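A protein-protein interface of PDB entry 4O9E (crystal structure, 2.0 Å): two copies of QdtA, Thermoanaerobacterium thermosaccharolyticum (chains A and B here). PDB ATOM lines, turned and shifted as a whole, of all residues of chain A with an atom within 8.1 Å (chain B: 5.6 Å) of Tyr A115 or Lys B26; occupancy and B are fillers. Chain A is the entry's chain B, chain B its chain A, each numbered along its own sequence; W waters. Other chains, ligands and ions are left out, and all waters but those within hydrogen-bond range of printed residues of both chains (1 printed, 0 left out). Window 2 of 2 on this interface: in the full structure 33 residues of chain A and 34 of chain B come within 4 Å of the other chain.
Printed residues of chain B within 4 Å of Tyr A115: Glu B24, Gly B25, Lys B26 and Ile B27. Printed residues of chain A within 4 Å of Lys B26: Tyr A115. Gly B25 touches just these residues of chain A: Lys A34 and Tyr A115. Of the printed residues of chain B, Arg A35 touches Glu B24 (3.8 Å). Of the printed residues of chain A, Glu B24 touches Lys A34, Arg A35, Tyr A115 and Tyr A116. Printed residues of chain B within 4 Å of Tyr A116: Glu B24 (2.8 Å). Of the printed residues of chain A, Ile B27 touches Tyr A115 (3.6 Å). Of the printed residues of chain B, Lys A34 touches Glu B24 (3.7 Å) and Gly B25 (3.0 Å). The nearest printed residue of chain B that does not touch Tyr A115 is Asp B32 (5.0 Å). The nearest printed residue of chain A that does not touch Lys B26 is Lys A34 (6.1 Å).
The side-chain carboxylate (OD2) of Asp B28 sits at hydrogen-bond distance from the backbone NH (N) of Glu B24, at 2.8 Å. The backbone carbonyl oxygen (O) of Phe B31 sits at hydrogen-bond distance from the backbone NH (N) of Lys B26 (2.8 Å). N of Lys A34 lies within hydrogen-bond range of O of Ala A112, at 3.0 Å. The backbone carbonyl oxygen (O) of Arg A35 sits at hydrogen-bond distance from the backbone NH (N) of Ala A112, at 2.9 Å. The guanidinium group (NE) of Arg A35 is in hydrogen-bond range of the backbone carbonyl oxygen (O) of Glu A114. The side-chain carboxylate of Glu A118 is in hydrogen-bond range of the side-chain hydroxyl of Tyr A116, at 2.5 Å.
Among the printed residues, merely in contact across the chains: Tyr A115 with Glu B24 (3.3 Å), Tyr A115 with Ile B27 (3.6 Å), Lys A34 with Glu B24 (3.7 Å), Arg A35 with Glu B24 (3.8 Å) and Tyr A115 with Lys B26 (3.996 Å).
Position printed for both chains: 32.
Of the 16 printed residues of chain A, 4 touch a printed residue of chain B. Printed residues of chain A that touch a printed residue of chain B: Lys A34, Arg A35, Tyr A115 and Tyr A116. Hydrophobic or aromatic side chains of chain B that line the printed part of chain A: Ile B27. Among the printed residues, no Asp or Glu carboxylate lies within 4 Å of a Lys or Arg side-chain nitrogen of the other chain.
Water W1 bridges the backbone carbonyl oxygen (O) of Tyr A116 (2.6 Å) and the side-chain carboxylate (OE2) of Glu B24 (2.8 Å).
OE2 of Glu B24 lies within hydrogen-bond range of N of Tyr A116 (2.8 Å). The backbone NH (N) of Gly B25 lies within hydrogen-bond range of the backbone carbonyl oxygen (O) of Lys A34 (3.0 Å). The backbone carbonyl oxygen (O) of Gly B25 is in hydrogen-bond range of the side-chain hydroxyl (OH) of Tyr A115 (2.7 Å).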
ATOM      1  N   ASP A  32      24.627 -11.570  21.889  1.00  0.00           N
ATOM      2  CA  ASP A  32      25.824 -12.399  21.824  1.00  0.00           C
ATOM      3  C   ASP A  32      26.724 -11.833  20.746  1.00  0.00           C
ATOM      4  O   ASP A  32      26.232 -11.342  19.717  1.00  0.00           O
ATOM      5  CB  ASP A  32      25.458 -13.817  21.410  1.00  0.00           C
ATOM      6  CG  ASP A  32      25.381 -14.724  22.609  1.00  0.00           C
ATOM      7  OD1 ASP A  32      26.347 -14.729  23.405  1.00  0.00           O
ATOM      8  OD2 ASP A  32      24.328 -15.364  22.775  1.00  0.00           O
ATOM      9  N   ILE A  33      28.026 -11.858  21.003  1.00  0.00           N
ATOM     10  CA  ILE A  33      28.974 -11.327  20.019  1.00  0.00           C
ATOM     11  C   ILE A  33      29.316 -12.388  18.994  1.00  0.00           C
ATOM     12  O   ILE A  33      30.078 -13.312  19.293  1.00  0.00           O
ATOM     13  CB  ILE A  33      30.267 -10.845  20.700  1.00  0.00           C
ATOM     14  CG1 ILE A  33      29.862  -9.794  21.731  1.00  0.00           C
ATOM     15  CG2 ILE A  33      31.218 -10.246  19.675  1.00  0.00           C
ATOM     16  CD1 ILE A  33      30.997  -9.451  22.655  1.00  0.00           C
ATOM     17  N   LYS A  34      28.796 -12.286  17.774  1.00  0.00           N
ATOM     18  CA  LYS A  34      29.211 -13.208  16.715  1.00  0.00           C
ATOM     19  C   LYS A  34      30.443 -12.767  15.937  1.00  0.00           C
ATOM     20  O   LYS A  34      31.107 -13.510  15.194  1.00  0.00           O
ATOM     21  CB  LYS A  34      28.020 -13.482  15.786  1.00  0.00           C
ATOM     22  CG  LYS A  34      27.000 -14.309  16.568  1.00  0.00           C
ATOM     23  CD  LYS A  34      25.919 -14.966  15.725  1.00  0.00           C
ATOM     24  CE  LYS A  34      25.068 -15.951  16.524  1.00  0.00           C
ATOM     25  NZ  LYS A  34      25.091 -15.905  18.021  1.00  0.00           N
ATOM     26  N   ARG A  35      30.637 -11.460  15.987  1.00  0.00           N
ATOM     27  CA  ARG A  35      31.669 -10.849  15.138  1.00  0.00           C
ATOM     28  C   ARG A  35      32.093  -9.541  15.777  1.00  0.00           C
ATOM     29  O   ARG A  35      31.267  -8.829  16.378  1.00  0.00           O
ATOM     30  CB  ARG A  35      31.092 -10.609  13.734  1.00  0.00           C
ATOM     31  CG  ARG A  35      31.900  -9.645  12.868  1.00  0.00           C
ATOM     32  CD  ARG A  35      31.389  -9.432  11.454  1.00  0.00           C
ATOM     33  NE  ARG A  35      29.956  -9.163  11.455  1.00  0.00           N
ATOM     34  CZ  ARG A  35      29.343  -8.102  10.937  1.00  0.00           C
ATOM     35  NH1 ARG A  35      28.014  -8.032  11.012  1.00  0.00           N
ATOM     36  NH2 ARG A  35      30.039  -7.156  10.317  1.00  0.00           N
ATOM     37  N   VAL A  36      33.388  -9.248  15.641  1.00  0.00           N
ATOM     38  CA  VAL A  36      33.877  -7.910  15.942  1.00  0.00           C
ATOM     39  C   VAL A  36      34.568  -7.365  14.692  1.00  0.00           C
ATOM     40  O   VAL A  36      35.028  -8.101  13.814  1.00  0.00           O
ATOM     41  CB  VAL A  36      34.797  -7.829  17.178  1.00  0.00           C
ATOM     42  CG1 VAL A  36      34.132  -8.413  18.413  1.00  0.00           C
ATOM     43  CG2 VAL A  36      36.087  -8.579  16.969  1.00  0.00           C
ATOM     44  N   HIS A  53      21.162  -1.295   8.616  1.00  0.00           N
ATOM     45  CA  HIS A  53      20.889  -2.730   8.574  1.00  0.00           C
ATOM     46  C   HIS A  53      19.449  -2.994   8.948  1.00  0.00           C
ATOM     47  O   HIS A  53      18.800  -2.269   9.719  1.00  0.00           O
ATOM     48  CB  HIS A  53      21.755  -3.460   9.587  1.00  0.00           C
ATOM     49  CG  HIS A  53      23.186  -3.550   9.169  1.00  0.00           C
ATOM     50  ND1 HIS A  53      24.106  -2.580   9.496  1.00  0.00           N
ATOM     51  CD2 HIS A  53      23.871  -4.522   8.517  1.00  0.00           C
ATOM     52  CE1 HIS A  53      25.284  -2.912   9.004  1.00  0.00           C
ATOM     53  NE2 HIS A  53      25.173  -4.095   8.420  1.00  0.00           N
ATOM     54  N   LEU A  56      20.661  -6.586  11.999  1.00  0.00           N
ATOM     55  CA  LEU A  56      21.816  -6.577  12.867  1.00  0.00           C
ATOM     56  C   LEU A  56      21.680  -5.608  14.041  1.00  0.00           C
ATOM     57  O   LEU A  56      21.177  -4.494  13.887  1.00  0.00           O
ATOM     58  CB  LEU A  56      22.998  -6.181  11.997  1.00  0.00           C
ATOM     59  CG  LEU A  56      24.368  -6.118  12.651  1.00  0.00           C
ATOM     60  CD1 LEU A  56      24.794  -7.576  12.828  1.00  0.00           C
ATOM     61  CD2 LEU A  56      25.372  -5.365  11.797  1.00  0.00           C
ATOM     62  N   ALA A 112      29.176  -6.905  16.911  1.00  0.00           N
ATOM     63  CA  ALA A 112      28.024  -7.253  16.113  1.00  0.00           C
ATOM     64  C   ALA A 112      27.341  -8.586  16.450  1.00  0.00           C
ATOM     65  O   ALA A 112      27.987  -9.624  16.680  1.00  0.00           O
ATOM     66  CB  ALA A 112      28.505  -7.221  14.679  1.00  0.00           C
ATOM     67  N   SER A 113      26.017  -8.552  16.360  1.00  0.00           N
ATOM     68  CA  SER A 113      25.140  -9.677  16.702  1.00  0.00           C
ATOM     69  C   SER A 113      25.093 -10.809  15.696  1.00  0.00           C
ATOM     70  O   SER A 113      24.554 -11.868  16.017  1.00  0.00           O
ATOM     71  CB  SER A 113      23.715  -9.246  17.074  1.00  0.00           C
ATOM     72  OG  SER A 113      22.967  -8.775  15.956  1.00  0.00           O
ATOM     73  N   GLU A 114      25.609 -10.580  14.493  1.00  0.00           N
ATOM     74  CA  GLU A 114      25.558 -11.538  13.381  1.00  0.00           C
ATOM     75  C   GLU A 114      26.821 -11.500  12.543  1.00  0.00           C
ATOM     76  O   GLU A 114      27.601 -10.526  12.534  1.00  0.00           O
ATOM     77  CB  GLU A 114      24.309 -11.318  12.517  1.00  0.00           C
ATOM     78  CG  GLU A 114      22.962 -11.358  13.218  1.00  0.00           C
ATOM     79  CD  GLU A 114      22.548 -12.738  13.722  1.00  0.00           C
ATOM     80  OE1 GLU A 114      23.160 -13.753  13.323  1.00  0.00           O
ATOM     81  OE2 GLU A 114      21.614 -12.760  14.544  1.00  0.00           O
ATOM     82  N   TYR A 115      27.099 -12.631  11.897  1.00  0.00           N
ATOM     83  CA  TYR A 115      28.142 -12.635  10.902  1.00  0.00           C
ATOM     84  C   TYR A 115      27.816 -11.640   9.773  1.00  0.00           C
ATOM     85  O   TYR A 115      26.648 -11.317   9.513  1.00  0.00           O
ATOM     86  CB  TYR A 115      28.292 -14.023  10.284  1.00  0.00           C
ATOM     87  CG  TYR A 115      28.851 -15.108  11.176  1.00  0.00           C
ATOM     88  CD1 TYR A 115      28.483 -16.432  10.967  1.00  0.00           C
ATOM     89  CD2 TYR A 115      29.739 -14.833  12.214  1.00  0.00           C
ATOM     90  CE1 TYR A 115      29.010 -17.454  11.734  1.00  0.00           C
ATOM     91  CE2 TYR A 115      30.211 -15.846  13.032  1.00  0.00           C
ATOM     92  CZ  TYR A 115      29.864 -17.156  12.774  1.00  0.00           C
ATOM     93  OH  TYR A 115      30.381 -18.192  13.523  1.00  0.00           O
ATOM     94  N   TYR A 116      28.873 -11.203   9.095  1.00  0.00           N
ATOM     95  CA  TYR A 116      28.767 -10.290   7.956  1.00  0.00           C
ATOM     96  C   TYR A 116      27.849 -10.924   6.932  1.00  0.00           C
ATOM     97  O   TYR A 116      28.046 -12.063   6.531  1.00  0.00           O
ATOM     98  CB  TYR A 116      30.102  -9.991   7.285  1.00  0.00           C
ATOM     99  CG  TYR A 116      30.025  -9.183   6.003  1.00  0.00           C
ATOM    100  CD1 TYR A 116      29.697  -7.830   6.033  1.00  0.00           C
ATOM    101  CD2 TYR A 116      30.353  -9.749   4.772  1.00  0.00           C
ATOM    102  CE1 TYR A 116      29.614  -7.083   4.871  1.00  0.00           C
ATOM    103  CE2 TYR A 116      30.305  -9.004   3.605  1.00  0.00           C
ATOM    104  CZ  TYR A 116      29.922  -7.675   3.663  1.00  0.00           C
ATOM    105  OH  TYR A 116      29.846  -6.881   2.542  1.00  0.00           O
ATOM    106  N   ASP A 117      26.820 -10.160   6.598  1.00  0.00           N
ATOM    107  CA  ASP A 117      25.852 -10.468   5.544  1.00  0.00           C
ATOM    108  C   ASP A 117      25.526  -9.207   4.726  1.00  0.00           C
ATOM    109  O   ASP A 117      24.714  -8.376   5.142  1.00  0.00           O
ATOM    110  CB  ASP A 117      24.584 -10.979   6.226  1.00  0.00           C
ATOM    111  CG  ASP A 117      23.499 -11.357   5.233  1.00  0.00           C
ATOM    112  OD1 ASP A 117      23.737 -11.273   4.010  1.00  0.00           O
ATOM    113  OD2 ASP A 117      22.404 -11.719   5.713  1.00  0.00           O
ATOM    114  N   GLU A 118      26.160  -9.077   3.566  1.00  0.00           N
ATOM    115  CA  GLU A 118      25.921  -7.961   2.665  1.00  0.00           C
ATOM    116  C   GLU A 118      24.437  -7.734   2.388  1.00  0.00           C
ATOM    117  O   GLU A 118      24.012  -6.583   2.390  1.00  0.00           O
ATOM    118  CB  GLU A 118      26.738  -8.085   1.376  1.00  0.00           C
ATOM    119  CG  GLU A 118      26.582  -6.878   0.460  1.00  0.00           C
ATOM    120  CD  GLU A 118      27.008  -5.548   1.067  1.00  0.00           C
ATOM    121  OE1 GLU A 118      27.886  -5.505   1.954  1.00  0.00           O
ATOM    122  OE2 GLU A 118      26.463  -4.495   0.662  1.00  0.00           O
ATOM    123  N   ASP A 120      21.986  -7.935   4.326  1.00  0.00           N
ATOM    124  CA  ASP A 120      21.285  -7.259   5.422  1.00  0.00           C
ATOM    125  C   ASP A 120      21.566  -5.757   5.441  1.00  0.00           C
ATOM    126  O   ASP A 120      20.927  -5.047   6.211  1.00  0.00           O
ATOM    127  CB  ASP A 120      21.620  -7.925   6.761  1.00  0.00           C
ATOM    128  CG  ASP A 120      20.967  -7.269   7.966  1.00  0.00           C
ATOM    129  OD1 ASP A 120      19.734  -7.229   8.113  1.00  0.00           O
ATOM    130  OD2 ASP A 120      21.720  -6.733   8.805  1.00  0.00           O
ATOM    131  N   TYR A 121      22.522  -5.297   4.637  1.00  0.00           N
ATOM    132  CA  TYR A 121      22.797  -3.866   4.509  1.00  0.00           C
ATOM    133  C   TYR A 121      21.843  -3.183   3.541  1.00  0.00           C
ATOM    134  O   TYR A 121      21.506  -3.742   2.499  1.00  0.00           O
ATOM    135  CB  TYR A 121      24.143  -3.590   3.854  1.00  0.00           C
ATOM    136  CG  TYR A 121      25.394  -3.672   4.691  1.00  0.00           C
ATOM    137  CD1 TYR A 121      25.911  -4.899   5.080  1.00  0.00           C
ATOM    138  CD2 TYR A 121      26.134  -2.531   4.982  1.00  0.00           C
ATOM    139  CE1 TYR A 121      27.135  -4.975   5.721  1.00  0.00           C
ATOM    140  CE2 TYR A 121      27.359  -2.601   5.619  1.00  0.00           C
ATOM    141  CZ  TYR A 121      27.861  -3.828   5.994  1.00  0.00           C
ATOM    142  OH  TYR A 121      29.040  -3.899   6.713  1.00  0.00           O
ATOM    143  N   GLU B  24      35.271 -12.977  12.728  1.00  0.00           N
ATOM    144  CA  GLU B  24      34.033 -13.693  13.006  1.00  0.00           C
ATOM    145  C   GLU B  24      34.349 -14.897  13.875  1.00  0.00           C
ATOM    146  O   GLU B  24      35.214 -15.717  13.539  1.00  0.00           O
ATOM    147  CB  GLU B  24      33.402 -14.111  11.676  1.00  0.00           C
ATOM    148  CG  GLU B  24      32.920 -12.902  10.871  1.00  0.00           C
ATOM    149  CD  GLU B  24      32.212 -13.304   9.595  1.00  0.00           C
ATOM    150  OE1 GLU B  24      32.701 -14.234   8.923  1.00  0.00           O
ATOM    151  OE2 GLU B  24      31.165 -12.717   9.275  1.00  0.00           O
ATOM    152  N   GLY B  25      33.627 -15.038  14.982  1.00  0.00           N
ATOM    153  CA  GLY B  25      33.920 -16.190  15.832  1.00  0.00           C
ATOM    154  C   GLY B  25      33.781 -17.513  15.102  1.00  0.00           C
ATOM    155  O   GLY B  25      32.906 -17.662  14.252  1.00  0.00           O
ATOM    156  N   LYS B  26      34.643 -18.459  15.450  1.00  0.00           N
ATOM    157  CA  LYS B  26      34.701 -19.764  14.803  1.00  0.00           C
ATOM    158  C   LYS B  26      35.156 -19.719  13.357  1.00  0.00           C
ATOM    159  O   LYS B  26      35.519 -20.777  12.841  1.00  0.00           O
ATOM    160  CB  LYS B  26      33.355 -20.489  14.882  1.00  0.00           C
ATOM    161  CG  LYS B  26      33.002 -20.800  16.323  1.00  0.00           C
ATOM    162  CD  LYS B  26      31.962 -21.901  16.485  1.00  0.00           C
ATOM    163  CE  LYS B  26      30.730 -21.715  15.628  1.00  0.00           C
ATOM    164  NZ  LYS B  26      29.852 -22.917  15.701  1.00  0.00           N
ATOM    165  N   ILE B  27      35.251 -18.552  12.718  1.00  0.00           N
ATOM    166  CA  ILE B  27      35.734 -18.514  11.334  1.00  0.00           C
ATOM    167  C   ILE B  27      37.130 -17.929  11.236  1.00  0.00           C
ATOM    168  O   ILE B  27      38.057 -18.612  10.790  1.00  0.00           O
ATOM    169  CB  ILE B  27      34.760 -17.776  10.389  1.00  0.00           C
ATOM    170  CG1 ILE B  27      33.431 -18.526  10.414  1.00  0.00           C
ATOM    171  CG2 ILE B  27      35.289 -17.614   8.956  1.00  0.00           C
ATOM    172  CD1 ILE B  27      32.221 -17.684  10.084  1.00  0.00           C
ATOM    173  N   ASP B  28      37.267 -16.670  11.631  1.00  0.00           N
ATOM    174  CA  ASP B  28      38.590 -16.065  11.612  1.00  0.00           C
ATOM    175  C   ASP B  28      39.491 -16.491  12.764  1.00  0.00           C
ATOM    176  O   ASP B  28      40.723 -16.397  12.685  1.00  0.00           O
ATOM    177  CB  ASP B  28      38.450 -14.554  11.574  1.00  0.00           C
ATOM    178  CG  ASP B  28      37.788 -14.108  10.289  1.00  0.00           C
ATOM    179  OD1 ASP B  28      38.308 -14.429   9.205  1.00  0.00           O
ATOM    180  OD2 ASP B  28      36.653 -13.621  10.394  1.00  0.00           O
ATOM    181  N   ILE B  29      38.831 -16.907  13.843  1.00  0.00           N
ATOM    182  CA  ILE B  29      39.455 -17.525  14.989  1.00  0.00           C
ATOM    183  C   ILE B  29      38.710 -18.820  15.312  1.00  0.00           C
ATOM    184  O   ILE B  29      37.558 -18.987  14.914  1.00  0.00           O
ATOM    185  CB  ILE B  29      39.507 -16.588  16.211  1.00  0.00           C
ATOM    186  CG1 ILE B  29      38.073 -16.222  16.595  1.00  0.00           C
ATOM    187  CG2 ILE B  29      40.369 -15.348  15.988  1.00  0.00           C
ATOM    188  CD1 ILE B  29      37.970 -15.567  17.942  1.00  0.00           C
ATOM    189  N   PRO B  30      39.380 -19.754  16.001  1.00  0.00           N
ATOM    190  CA  PRO B  30      38.830 -21.110  16.147  1.00  0.00           C
ATOM    191  C   PRO B  30      37.703 -21.265  17.178  1.00  0.00           C
ATOM    192  O   PRO B  30      36.994 -22.270  17.168  1.00  0.00           O
ATOM    193  CB  PRO B  30      40.065 -21.972  16.470  1.00  0.00           C
ATOM    194  CG  PRO B  30      41.103 -21.030  16.980  1.00  0.00           C
ATOM    195  CD  PRO B  30      40.800 -19.687  16.367  1.00  0.00           C
ATOM    196  N   PHE B  31      37.425 -20.238  17.972  1.00  0.00           N
ATOM    197  CA  PHE B  31      36.435 -20.330  19.041  1.00  0.00           C
ATOM    198  C   PHE B  31      35.370 -19.243  18.911  1.00  0.00           C
ATOM    199  O   PHE B  31      35.543 -18.311  18.131  1.00  0.00           O
ATOM    200  CB  PHE B  31      37.158 -20.270  20.380  1.00  0.00           C
ATOM    201  CG  PHE B  31      38.014 -19.050  20.597  1.00  0.00           C
ATOM    202  CD1 PHE B  31      37.472 -17.893  21.110  1.00  0.00           C
ATOM    203  CD2 PHE B  31      39.384 -19.073  20.379  1.00  0.00           C
ATOM    204  CE1 PHE B  31      38.296 -16.828  21.413  1.00  0.00           C
ATOM    205  CE2 PHE B  31      40.189 -18.003  20.691  1.00  0.00           C
ATOM    206  CZ  PHE B  31      39.654 -16.847  21.185  1.00  0.00           C
ATOM    207  N   ASP B  32      34.249 -19.432  19.597  1.00  0.00           N
ATOM    208  CA  ASP B  32      33.207 -18.417  19.742  1.00  0.00           C
ATOM    209  C   ASP B  32      33.687 -17.319  20.684  1.00  0.00           C
ATOM    210  O   ASP B  32      34.268 -17.616  21.731  1.00  0.00           O
ATOM    211  CB  ASP B  32      31.925 -19.002  20.358  1.00  0.00           C
ATOM    212  CG  ASP B  32      31.086 -19.807  19.368  1.00  0.00           C
ATOM    213  OD1 ASP B  32      30.542 -19.225  18.417  1.00  0.00           O
ATOM    214  OD2 ASP B  32      30.916 -21.038  19.503  1.00  0.00           O
HETATM  215  O   HOH W   1      30.036 -13.658   6.905  1.00  0.00           O
